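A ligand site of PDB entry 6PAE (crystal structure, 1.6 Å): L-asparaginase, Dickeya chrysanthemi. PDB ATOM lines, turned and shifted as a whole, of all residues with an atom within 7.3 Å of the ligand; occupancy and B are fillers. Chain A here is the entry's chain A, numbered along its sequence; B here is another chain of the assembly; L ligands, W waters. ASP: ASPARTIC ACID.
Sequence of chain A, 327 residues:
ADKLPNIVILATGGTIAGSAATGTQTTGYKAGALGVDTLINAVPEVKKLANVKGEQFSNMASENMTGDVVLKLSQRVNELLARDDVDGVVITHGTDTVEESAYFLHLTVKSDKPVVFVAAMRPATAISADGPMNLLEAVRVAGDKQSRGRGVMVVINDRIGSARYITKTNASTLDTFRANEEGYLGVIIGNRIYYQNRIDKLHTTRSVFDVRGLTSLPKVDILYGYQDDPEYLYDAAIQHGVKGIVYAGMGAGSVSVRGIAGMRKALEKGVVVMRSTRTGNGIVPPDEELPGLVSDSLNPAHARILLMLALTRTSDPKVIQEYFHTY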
ATOM      1  N   GLY A  13      22.941  22.191  28.902  1.00  0.00           N
ATOM      2  CA  GLY A  13      22.547  21.381  30.035  1.00  0.00           C
ATOM      3  C   GLY A  13      22.907  19.900  29.871  1.00  0.00           C
ATOM      4  O   GLY A  13      23.951  19.581  29.239  1.00  0.00           O
ATOM      5  N   GLY A  14      22.073  19.003  30.457  1.00  0.00           N
ATOM      6  CA  GLY A  14      22.350  17.551  30.373  1.00  0.00           C
ATOM      7  C   GLY A  14      23.147  16.963  31.514  1.00  0.00           C
ATOM      8  O   GLY A  14      23.763  17.645  32.317  1.00  0.00           O
ATOM      9  N   THR A  15      23.077  15.655  31.571  1.00  0.00           N
ATOM     10  CA  THR A  15      23.884  14.861  32.535  1.00  0.00           C
ATOM     11  C   THR A  15      25.380  15.157  32.408  1.00  0.00           C
ATOM     12  O   THR A  15      26.113  15.050  33.386  1.00  0.00           O
ATOM     13  CB  THR A  15      23.574  13.390  32.372  1.00  0.00           C
ATOM     14  OG1 THR A  15      22.167  13.266  32.666  1.00  0.00           O
ATOM     15  CG2 THR A  15      24.478  12.500  33.229  1.00  0.00           C
ATOM     16  N   ILE A  16      25.846  15.549  31.214  1.00  0.00           N
ATOM     17  CA  ILE A  16      27.261  15.968  31.088  1.00  0.00           C
ATOM     18  C   ILE A  16      27.646  17.061  32.064  1.00  0.00           C
ATOM     19  O   ILE A  16      28.804  17.233  32.415  1.00  0.00           O
ATOM     20  CB  ILE A  16      27.623  16.352  29.634  1.00  0.00           C
ATOM     21  CG1 ILE A  16      29.089  16.532  29.466  1.00  0.00           C
ATOM     22  CG2 ILE A  16      26.751  17.516  29.109  1.00  0.00           C
ATOM     23  CD1 ILE A  16      29.525  16.560  27.995  1.00  0.00           C
ATOM     24  N   ALA A  17      26.616  17.858  32.411  1.00  0.00           N
ATOM     25  CA  ALA A  17      26.755  18.990  33.387  1.00  0.00           C
ATOM     26  C   ALA A  17      25.992  18.712  34.678  1.00  0.00           C
ATOM     27  O   ALA A  17      25.610  19.633  35.371  1.00  0.00           O
ATOM     28  CB  ALA A  17      26.302  20.266  32.720  1.00  0.00           C
ATOM     29  N   MET A  60      19.445  23.103  31.068  1.00  0.00           N
ATOM     30  CA  MET A  60      18.291  22.300  31.334  1.00  0.00           C
ATOM     31  C   MET A  60      18.508  20.852  30.970  1.00  0.00           C
ATOM     32  O   MET A  60      19.406  20.534  30.141  1.00  0.00           O
ATOM     33  CB  MET A  60      17.136  22.786  30.461  1.00  0.00           C
ATOM     34  CG  MET A  60      17.306  22.629  28.934  1.00  0.00           C
ATOM     35  SD  MET A  60      15.763  23.118  28.024  1.00  0.00           S
ATOM     36  CE  MET A  60      16.249  24.812  27.802  1.00  0.00           C
ATOM     37  N   ALA A  61      17.673  19.986  31.545  1.00  0.00           N
ATOM     38  CA  ALA A  61      17.656  18.594  31.186  1.00  0.00           C
ATOM     39  C   ALA A  61      17.020  18.515  29.762  1.00  0.00           C
ATOM     40  O   ALA A  61      16.052  19.261  29.482  1.00  0.00           O
ATOM     41  CB  ALA A  61      16.891  17.770  32.287  1.00  0.00           C
ATOM     42  N   SER A  62      17.577  17.634  28.870  1.00  0.00           N
ATOM     43  CA  SER A  62      17.147  17.659  27.464  1.00  0.00           C
ATOM     44  C   SER A  62      15.747  17.177  27.257  1.00  0.00           C
ATOM     45  O   SER A  62      15.133  17.559  26.310  1.00  0.00           O
ATOM     46  CB  SER A  62      18.056  16.911  26.503  1.00  0.00           C
ATOM     47  OG  SER A  62      17.996  15.510  26.720  1.00  0.00           O
ATOM     48  N   GLU A  63      15.179  16.479  28.192  1.00  0.00           N
ATOM     49  CA  GLU A  63      13.717  16.165  28.141  1.00  0.00           C
ATOM     50  C   GLU A  63      12.842  17.356  28.186  1.00  0.00           C
ATOM     51  O   GLU A  63      11.715  17.292  27.777  1.00  0.00           O
ATOM     52  CB  GLU A  63      13.295  15.175  29.257  1.00  0.00           C
ATOM     53  CG  GLU A  63      13.429  15.582  30.691  1.00  0.00           C
ATOM     54  CD  GLU A  63      14.788  15.307  31.340  1.00  0.00           C
ATOM     55  OE1 GLU A  63      15.852  15.217  30.566  1.00  0.00           O
ATOM     56  OE2 GLU A  63      14.718  15.077  32.587  1.00  0.00           O
ATOM     57  N   ASN A  64      13.388  18.457  28.720  1.00  0.00           N
ATOM     58  CA  ASN A  64      12.727  19.796  28.636  1.00  0.00           C
ATOM     59  C   ASN A  64      13.089  20.717  27.493  1.00  0.00           C
ATOM     60  O   ASN A  64      12.532  21.812  27.355  1.00  0.00           O
ATOM     61  CB  ASN A  64      12.920  20.463  30.008  1.00  0.00           C
ATOM     62  CG  ASN A  64      12.027  19.882  30.999  1.00  0.00           C
ATOM     63  OD1 ASN A  64      10.789  19.771  30.726  1.00  0.00           O
ATOM     64  ND2 ASN A  64      12.562  19.484  32.144  1.00  0.00           N
ATOM     65  N   HIS A  93      24.921  18.901  25.649  1.00  0.00           N
ATOM     66  CA  HIS A  93      23.463  18.704  25.693  1.00  0.00           C
ATOM     67  C   HIS A  93      23.173  17.405  26.426  1.00  0.00           C
ATOM     68  O   HIS A  93      24.028  16.504  26.518  1.00  0.00           O
ATOM     69  CB  HIS A  93      23.037  18.582  24.221  1.00  0.00           C
ATOM     70  CG  HIS A  93      21.577  18.720  23.891  1.00  0.00           C
ATOM     71  ND1 HIS A  93      20.654  17.700  24.058  1.00  0.00           N
ATOM     72  CD2 HIS A  93      20.915  19.701  23.232  1.00  0.00           C
ATOM     73  CE1 HIS A  93      19.496  18.064  23.571  1.00  0.00           C
ATOM     74  NE2 HIS A  93      19.607  19.284  23.049  1.00  0.00           N
ATOM     75  N   GLY A  94      21.941  17.267  26.917  1.00  0.00           N
ATOM     76  CA  GLY A  94      21.455  16.016  27.473  1.00  0.00           C
ATOM     77  C   GLY A  94      21.373  14.895  26.396  1.00  0.00           C
ATOM     78  O   GLY A  94      21.135  15.171  25.219  1.00  0.00           O
ATOM     79  N   THR A  95      21.590  13.653  26.784  1.00  0.00           N
ATOM     80  CA  THR A  95      21.496  12.509  25.844  1.00  0.00           C
ATOM     81  C   THR A  95      20.069  12.170  25.406  1.00  0.00           C
ATOM     82  O   THR A  95      19.844  11.766  24.231  1.00  0.00           O
ATOM     83  CB  THR A  95      22.039  11.230  26.471  1.00  0.00           C
ATOM     84  OG1 THR A  95      21.234  10.862  27.606  1.00  0.00           O
ATOM     85  CG2 THR A  95      23.533  11.357  26.871  1.00  0.00           C
ATOM     86  N   ASP A  96      19.088  12.544  26.228  1.00  0.00           N
ATOM     87  CA  ASP A  96      17.713  12.049  25.955  1.00  0.00           C
ATOM     88  C   ASP A  96      17.073  12.588  24.679  1.00  0.00           C
ATOM     89  O   ASP A  96      16.476  11.772  23.913  1.00  0.00           O
ATOM     90  CB  ASP A  96      16.741  12.312  27.124  1.00  0.00           C
ATOM     91  CG  ASP A  96      17.096  11.578  28.418  1.00  0.00           C
ATOM     92  OD1 ASP A  96      17.929  10.628  28.324  1.00  0.00           O
ATOM     93  OD2 ASP A  96      16.528  12.034  29.484  1.00  0.00           O
ATOM     94  N   THR A  97      17.342  13.838  24.317  1.00  0.00           N
ATOM     95  CA  THR A  97      16.800  14.365  23.085  1.00  0.00           C
ATOM     96  C   THR A  97      17.858  15.040  22.196  1.00  0.00           C
ATOM     97  O   THR A  97      17.520  15.845  21.243  1.00  0.00           O
ATOM     98  CB  THR A  97      15.667  15.415  23.311  1.00  0.00           C
ATOM     99  OG1 THR A  97      16.156  16.662  23.846  1.00  0.00           O
ATOM    100  CG2 THR A  97      14.532  14.873  24.200  1.00  0.00           C
ATOM    101  N   VAL A  98      19.119  14.700  22.419  1.00  0.00           N
ATOM    102  CA  VAL A  98      20.185  15.209  21.550  1.00  0.00           C
ATOM    103  C   VAL A  98      19.926  14.893  20.082  1.00  0.00           C
ATOM    104  O   VAL A  98      20.242  15.679  19.213  1.00  0.00           O
ATOM    105  CB  VAL A  98      21.577  14.787  22.033  1.00  0.00           C
ATOM    106  CG1 VAL A  98      21.864  13.304  21.759  1.00  0.00           C
ATOM    107  CG2 VAL A  98      22.663  15.623  21.348  1.00  0.00           C
ATOM    108  N   ALA A 119      27.531  14.756  24.664  1.00  0.00           N
ATOM    109  CA  ALA A 119      26.688  14.458  25.849  1.00  0.00           C
ATOM    110  C   ALA A 119      27.407  13.421  26.680  1.00  0.00           C
ATOM    111  O   ALA A 119      28.567  13.002  26.293  1.00  0.00           O
ATOM    112  CB  ALA A 119      25.318  13.955  25.377  1.00  0.00           C
ATOM    113  N   ALA A 120      26.771  13.016  27.774  1.00  0.00           N
ATOM    114  CA  ALA A 120      27.379  12.029  28.675  1.00  0.00           C
ATOM    115  C   ALA A 120      26.258  11.290  29.386  1.00  0.00           C
ATOM    116  O   ALA A 120      25.268  11.942  29.804  1.00  0.00           O
ATOM    117  CB  ALA A 120      28.230  12.757  29.658  1.00  0.00           C
ATOM    118  N   MET A 121      26.421   9.975  29.515  1.00  0.00           N
ATOM    119  CA  MET A 121      25.483   9.115  30.124  1.00  0.00           C
ATOM    120  C   MET A 121      25.637   9.030  31.631  1.00  0.00           C
ATOM    121  O   MET A 121      24.628   8.746  32.309  1.00  0.00           O
ATOM    122  CB  MET A 121      25.532   7.765  29.450  1.00  0.00           C
ATOM    123  CG  MET A 121      24.871   7.713  28.103  1.00  0.00           C
ATOM    124  SD  MET A 121      23.109   7.938  28.168  1.00  0.00           S
ATOM    125  CE  MET A 121      22.645   6.405  28.914  1.00  0.00           C
ATOM    126  N   ARG A 122      26.818   9.391  32.144  1.00  0.00           N
ATOM    127  CA  ARG A 122      27.071   9.446  33.573  1.00  0.00           C
ATOM    128  C   ARG A 122      27.307  10.906  33.966  1.00  0.00           C
ATOM    129  O   ARG A 122      27.938  11.637  33.221  1.00  0.00           O
ATOM    130  CB  ARG A 122      28.295   8.604  33.917  1.00  0.00           C
ATOM    131  CG  ARG A 122      28.055   7.109  33.887  1.00  0.00           C
ATOM    132  CD  ARG A 122      29.352   6.322  33.946  1.00  0.00           C
ATOM    133  NE  ARG A 122      29.127   4.876  33.701  1.00  0.00           N
ATOM    134  CZ  ARG A 122      30.101   4.010  33.554  1.00  0.00           C
ATOM    135  NH1 ARG A 122      31.354   4.376  33.588  1.00  0.00           N
ATOM    136  NH2 ARG A 122      29.820   2.719  33.354  1.00  0.00           N
ATOM    137  N   PRO A 123      26.817  11.320  35.151  1.00  0.00           N
ATOM    138  CA  PRO A 123      27.121  12.669  35.581  1.00  0.00           C
ATOM    139  C   PRO A 123      28.608  12.925  35.840  1.00  0.00           C
ATOM    140  O   PRO A 123      29.422  12.015  36.016  1.00  0.00           O
ATOM    141  CB  PRO A 123      26.257  12.827  36.845  1.00  0.00           C
ATOM    142  CG  PRO A 123      26.182  11.434  37.408  1.00  0.00           C
ATOM    143  CD  PRO A 123      26.220  10.491  36.199  1.00  0.00           C
ATOM    144  N   LYS A 168      19.582   7.428  20.394  1.00  0.00           N
ATOM    145  CA  LYS A 168      19.808   6.789  21.723  1.00  0.00           C
ATOM    146  C   LYS A 168      19.000   5.468  21.679  1.00  0.00           C
ATOM    147  O   LYS A 168      17.750   5.473  21.574  1.00  0.00           O
ATOM    148  CB  LYS A 168      19.375   7.732  22.854  1.00  0.00           C
ATOM    149  CG  LYS A 168      19.696   7.177  24.249  1.00  0.00           C
ATOM    150  CD  LYS A 168      19.335   8.161  25.359  1.00  0.00           C
ATOM    151  CE  LYS A 168      19.742   7.617  26.716  1.00  0.00           C
ATOM    152  NZ  LYS A 168      19.721   8.601  27.775  1.00  0.00           N
ATOM    153  N   ALA A 171      18.322   2.845  27.188  1.00  0.00           N
ATOM    154  CA  ALA A 171      18.020   3.772  28.306  1.00  0.00           C
ATOM    155  C   ALA A 171      19.209   4.267  29.066  1.00  0.00           C
ATOM    156  O   ALA A 171      19.256   5.427  29.436  1.00  0.00           O
ATOM    157  CB  ALA A 171      17.006   3.171  29.263  1.00  0.00           C
ATOM    158  N   PHE A 177      24.374   5.252  21.923  1.00  0.00           N
ATOM    159  CA  PHE A 177      24.234   5.887  20.600  1.00  0.00           C
ATOM    160  C   PHE A 177      24.767   5.010  19.511  1.00  0.00           C
ATOM    161  O   PHE A 177      25.959   4.708  19.503  1.00  0.00           O
ATOM    162  CB  PHE A 177      24.861   7.285  20.581  1.00  0.00           C
ATOM    163  CG  PHE A 177      24.056   8.299  21.384  1.00  0.00           C
ATOM    164  CD1 PHE A 177      22.971   8.862  20.774  1.00  0.00           C
ATOM    165  CD2 PHE A 177      24.333   8.561  22.735  1.00  0.00           C
ATOM    166  CE1 PHE A 177      22.154   9.737  21.409  1.00  0.00           C
ATOM    167  CE2 PHE A 177      23.499   9.453  23.420  1.00  0.00           C
ATOM    168  CZ  PHE A 177      22.430  10.044  22.760  1.00  0.00           C
ATOM    169  N   MET B 250      11.495   9.480  26.901  1.00  0.00           N
ATOM    170  CA  MET B 250      12.794   9.883  26.444  1.00  0.00           C
ATOM    171  C   MET B 250      13.872   9.244  27.320  1.00  0.00           C
ATOM    172  O   MET B 250      13.760   9.219  28.561  1.00  0.00           O
ATOM    173  CB  MET B 250      12.919  11.452  26.481  1.00  0.00           C
ATOM    174  CG  MET B 250      11.951  12.126  25.512  1.00  0.00           C
ATOM    175  SD  MET B 250      11.747  13.901  25.823  1.00  0.00           S
ATOM    176  CE  MET B 250      10.418  13.864  27.054  1.00  0.00           C
ATOM    177  N   GLY B 251      14.941   8.711  26.723  1.00  0.00           N
ATOM    178  CA  GLY B 251      15.953   8.092  27.508  1.00  0.00           C
ATOM    179  C   GLY B 251      15.488   7.056  28.523  1.00  0.00           C
ATOM    180  O   GLY B 251      14.637   6.176  28.219  1.00  0.00           O
ATOM    181  N   ALA B 252      15.918   7.233  29.774  1.00  0.00           N
ATOM    182  CA  ALA B 252      15.603   6.232  30.842  1.00  0.00           C
ATOM    183  C   ALA B 252      14.322   6.697  31.533  1.00  0.00           C
ATOM    184  O   ALA B 252      14.232   6.950  32.772  1.00  0.00           O
ATOM    185  CB  ALA B 252      16.805   6.164  31.745  1.00  0.00           C
ATOM    186  N   SER B 254      12.688   9.435  31.218  1.00  0.00           N
ATOM    187  CA  SER B 254      12.750  10.832  31.590  1.00  0.00           C
ATOM    188  C   SER B 254      11.502  11.517  31.128  1.00  0.00           C
ATOM    189  O   SER B 254      10.983  11.235  30.103  1.00  0.00           O
ATOM    190  CB  SER B 254      13.956  11.564  30.973  1.00  0.00           C
ATOM    191  OG  SER B 254      15.098  10.877  31.417  1.00  0.00           O
ATOM    192  N   VAL B 255      11.062  12.473  31.923  1.00  0.00           N
ATOM    193  CA  VAL B 255       9.772  13.152  31.730  1.00  0.00           C
ATOM    194  C   VAL B 255       9.897  14.676  31.712  1.00  0.00           C
ATOM    195  O   VAL B 255      10.564  15.292  32.570  1.00  0.00           O
ATOM    196  CB  VAL B 255       8.788  12.734  32.847  1.00  0.00           C
ATOM    197  CG1 VAL B 255       7.343  13.142  32.452  1.00  0.00           C
ATOM    198  CG2 VAL B 255       8.855  11.260  33.249  1.00  0.00           C
HETATM  199  N   ASP L   1      17.921  13.322  31.325  1.00  0.00           N
HETATM  200  CA  ASP L   1      19.325  13.759  30.985  1.00  0.00           C
HETATM  201  C   ASP L   1      19.257  14.746  29.801  1.00  0.00           C
HETATM  202  O   ASP L   1      18.931  14.294  28.672  1.00  0.00           O
HETATM  203  CB  ASP L   1      20.013  12.429  30.565  1.00  0.00           C
HETATM  204  CG  ASP L   1      21.446  12.559  29.964  1.00  0.00           C
HETATM  205  OD1 ASP L   1      22.140  11.435  29.867  1.00  0.00           O
HETATM  206  OD2 ASP L   1      21.957  13.748  29.704  1.00  0.00           O
HETATM  207  OXT ASP L   1      19.468  15.914  30.012  1.00  0.00           O
HETATM  208  O   HOH W   1      22.055   9.555  31.620  1.00  0.00           O
HETATM  209  O   HOH W   2      18.477  11.950  33.838  1.00  0.00           O
HETATM  210  O   HOH W   3      16.908  14.622  33.889  1.00  0.00           O
HETATM  211  O   HOH W   4      24.547  14.742  28.714  1.00  0.00           O
HETATM  212  O   HOH W   5      20.091  16.713  33.018  1.00  0.00           O
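OG1 of Thr 15 sits close to OD2 of the ligand (3.0 Å). The backbone NH (N) of Thr 95 lies within hydrogen-bond range of an oxygen (OD2) of the ligand (2.9 Å). N of the ligand lies within salt-bridge range of OE1 of Glu 63 (2.9 Å). N of the ligand lies within salt-bridge range of OD2 of Asp 96. The side-chain hydroxyl of Thr 95 lies within hydrogen-bond range of an oxygen (OD1) of the ligand (2.5 Å). The backbone NH (N) of Asp 96 is in hydrogen-bond range of an oxygen (O) of the ligand (3.0 Å). An oxygen (OD2) of the ligand sits at hydrogen-bond distance from the backbone NH (N) of Thr 15 (2.9 Å). An oxygen (O) of the ligand lies within hydrogen-bond range of the side-chain hydroxyl (OG) of Ser 62, at 2.5 Å. N of Ser 62 lies within hydrogen-bond range of OXT of the ligand (2.8 Å).
The side-chain hydroxyl (OG) of Ser 62 lies close to the backbone carbonyl oxygen (O) of Gly 94 (3.5 Å). The side-chain hydroxyl (OG1) of Thr 95 lies within hydrogen-bond range of the side-chain carboxylate (OD1) of Asp 96 (3.4 Å). N of Gly 14 lies within hydrogen-bond range of O of Met 60 (3.1 Å). The side-chain hydroxyl (OG) of Ser 62 is in hydrogen-bond range of the backbone NH (N) of Asp 96 (3.2 Å). The side-chain carboxylate of Asp 96 sits at hydrogen-bond distance from the side-chain hydroxyl of Ser 254 of chain B. The side-chain amino group of Lys 168 is in hydrogen-bond range of the side-chain hydroxyl of Thr 95, at 2.7 Å. OG1 of Thr 95 lies within hydrogen-bond range of SD of Met 121 (3.5 Å). OD1 of Asp 96 lies within salt-bridge range of NZ of Lys 168.
The backbone carbonyl oxygen of Ala 120 sits close to an oxygen (OD1) of the ligand, at 3.2 Å. Merely in contact with the ligand: Gly 14 (3.3 Å), Ala 61 (3.4 Å), Gly 94 (3.2 Å) and Ser 254 of chain B (3.7 Å). Of the 29 residues printed, 10 come within 4 Å of the ligand. The nearest printed residue that does not touch the ligand is Met 121 (4.01 Å).
Water W1 bridges an oxygen (OD1) of the ligand (2.6 Å) and the backbone carbonyl oxygen (O) of Met 121 (2.8 Å). Water W3 bridges OE2 of Glu 63 and N of the ligand. Water W5 bridges OXT of the ligand (3.2 Å) and N of Thr 15 (3.5 Å).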
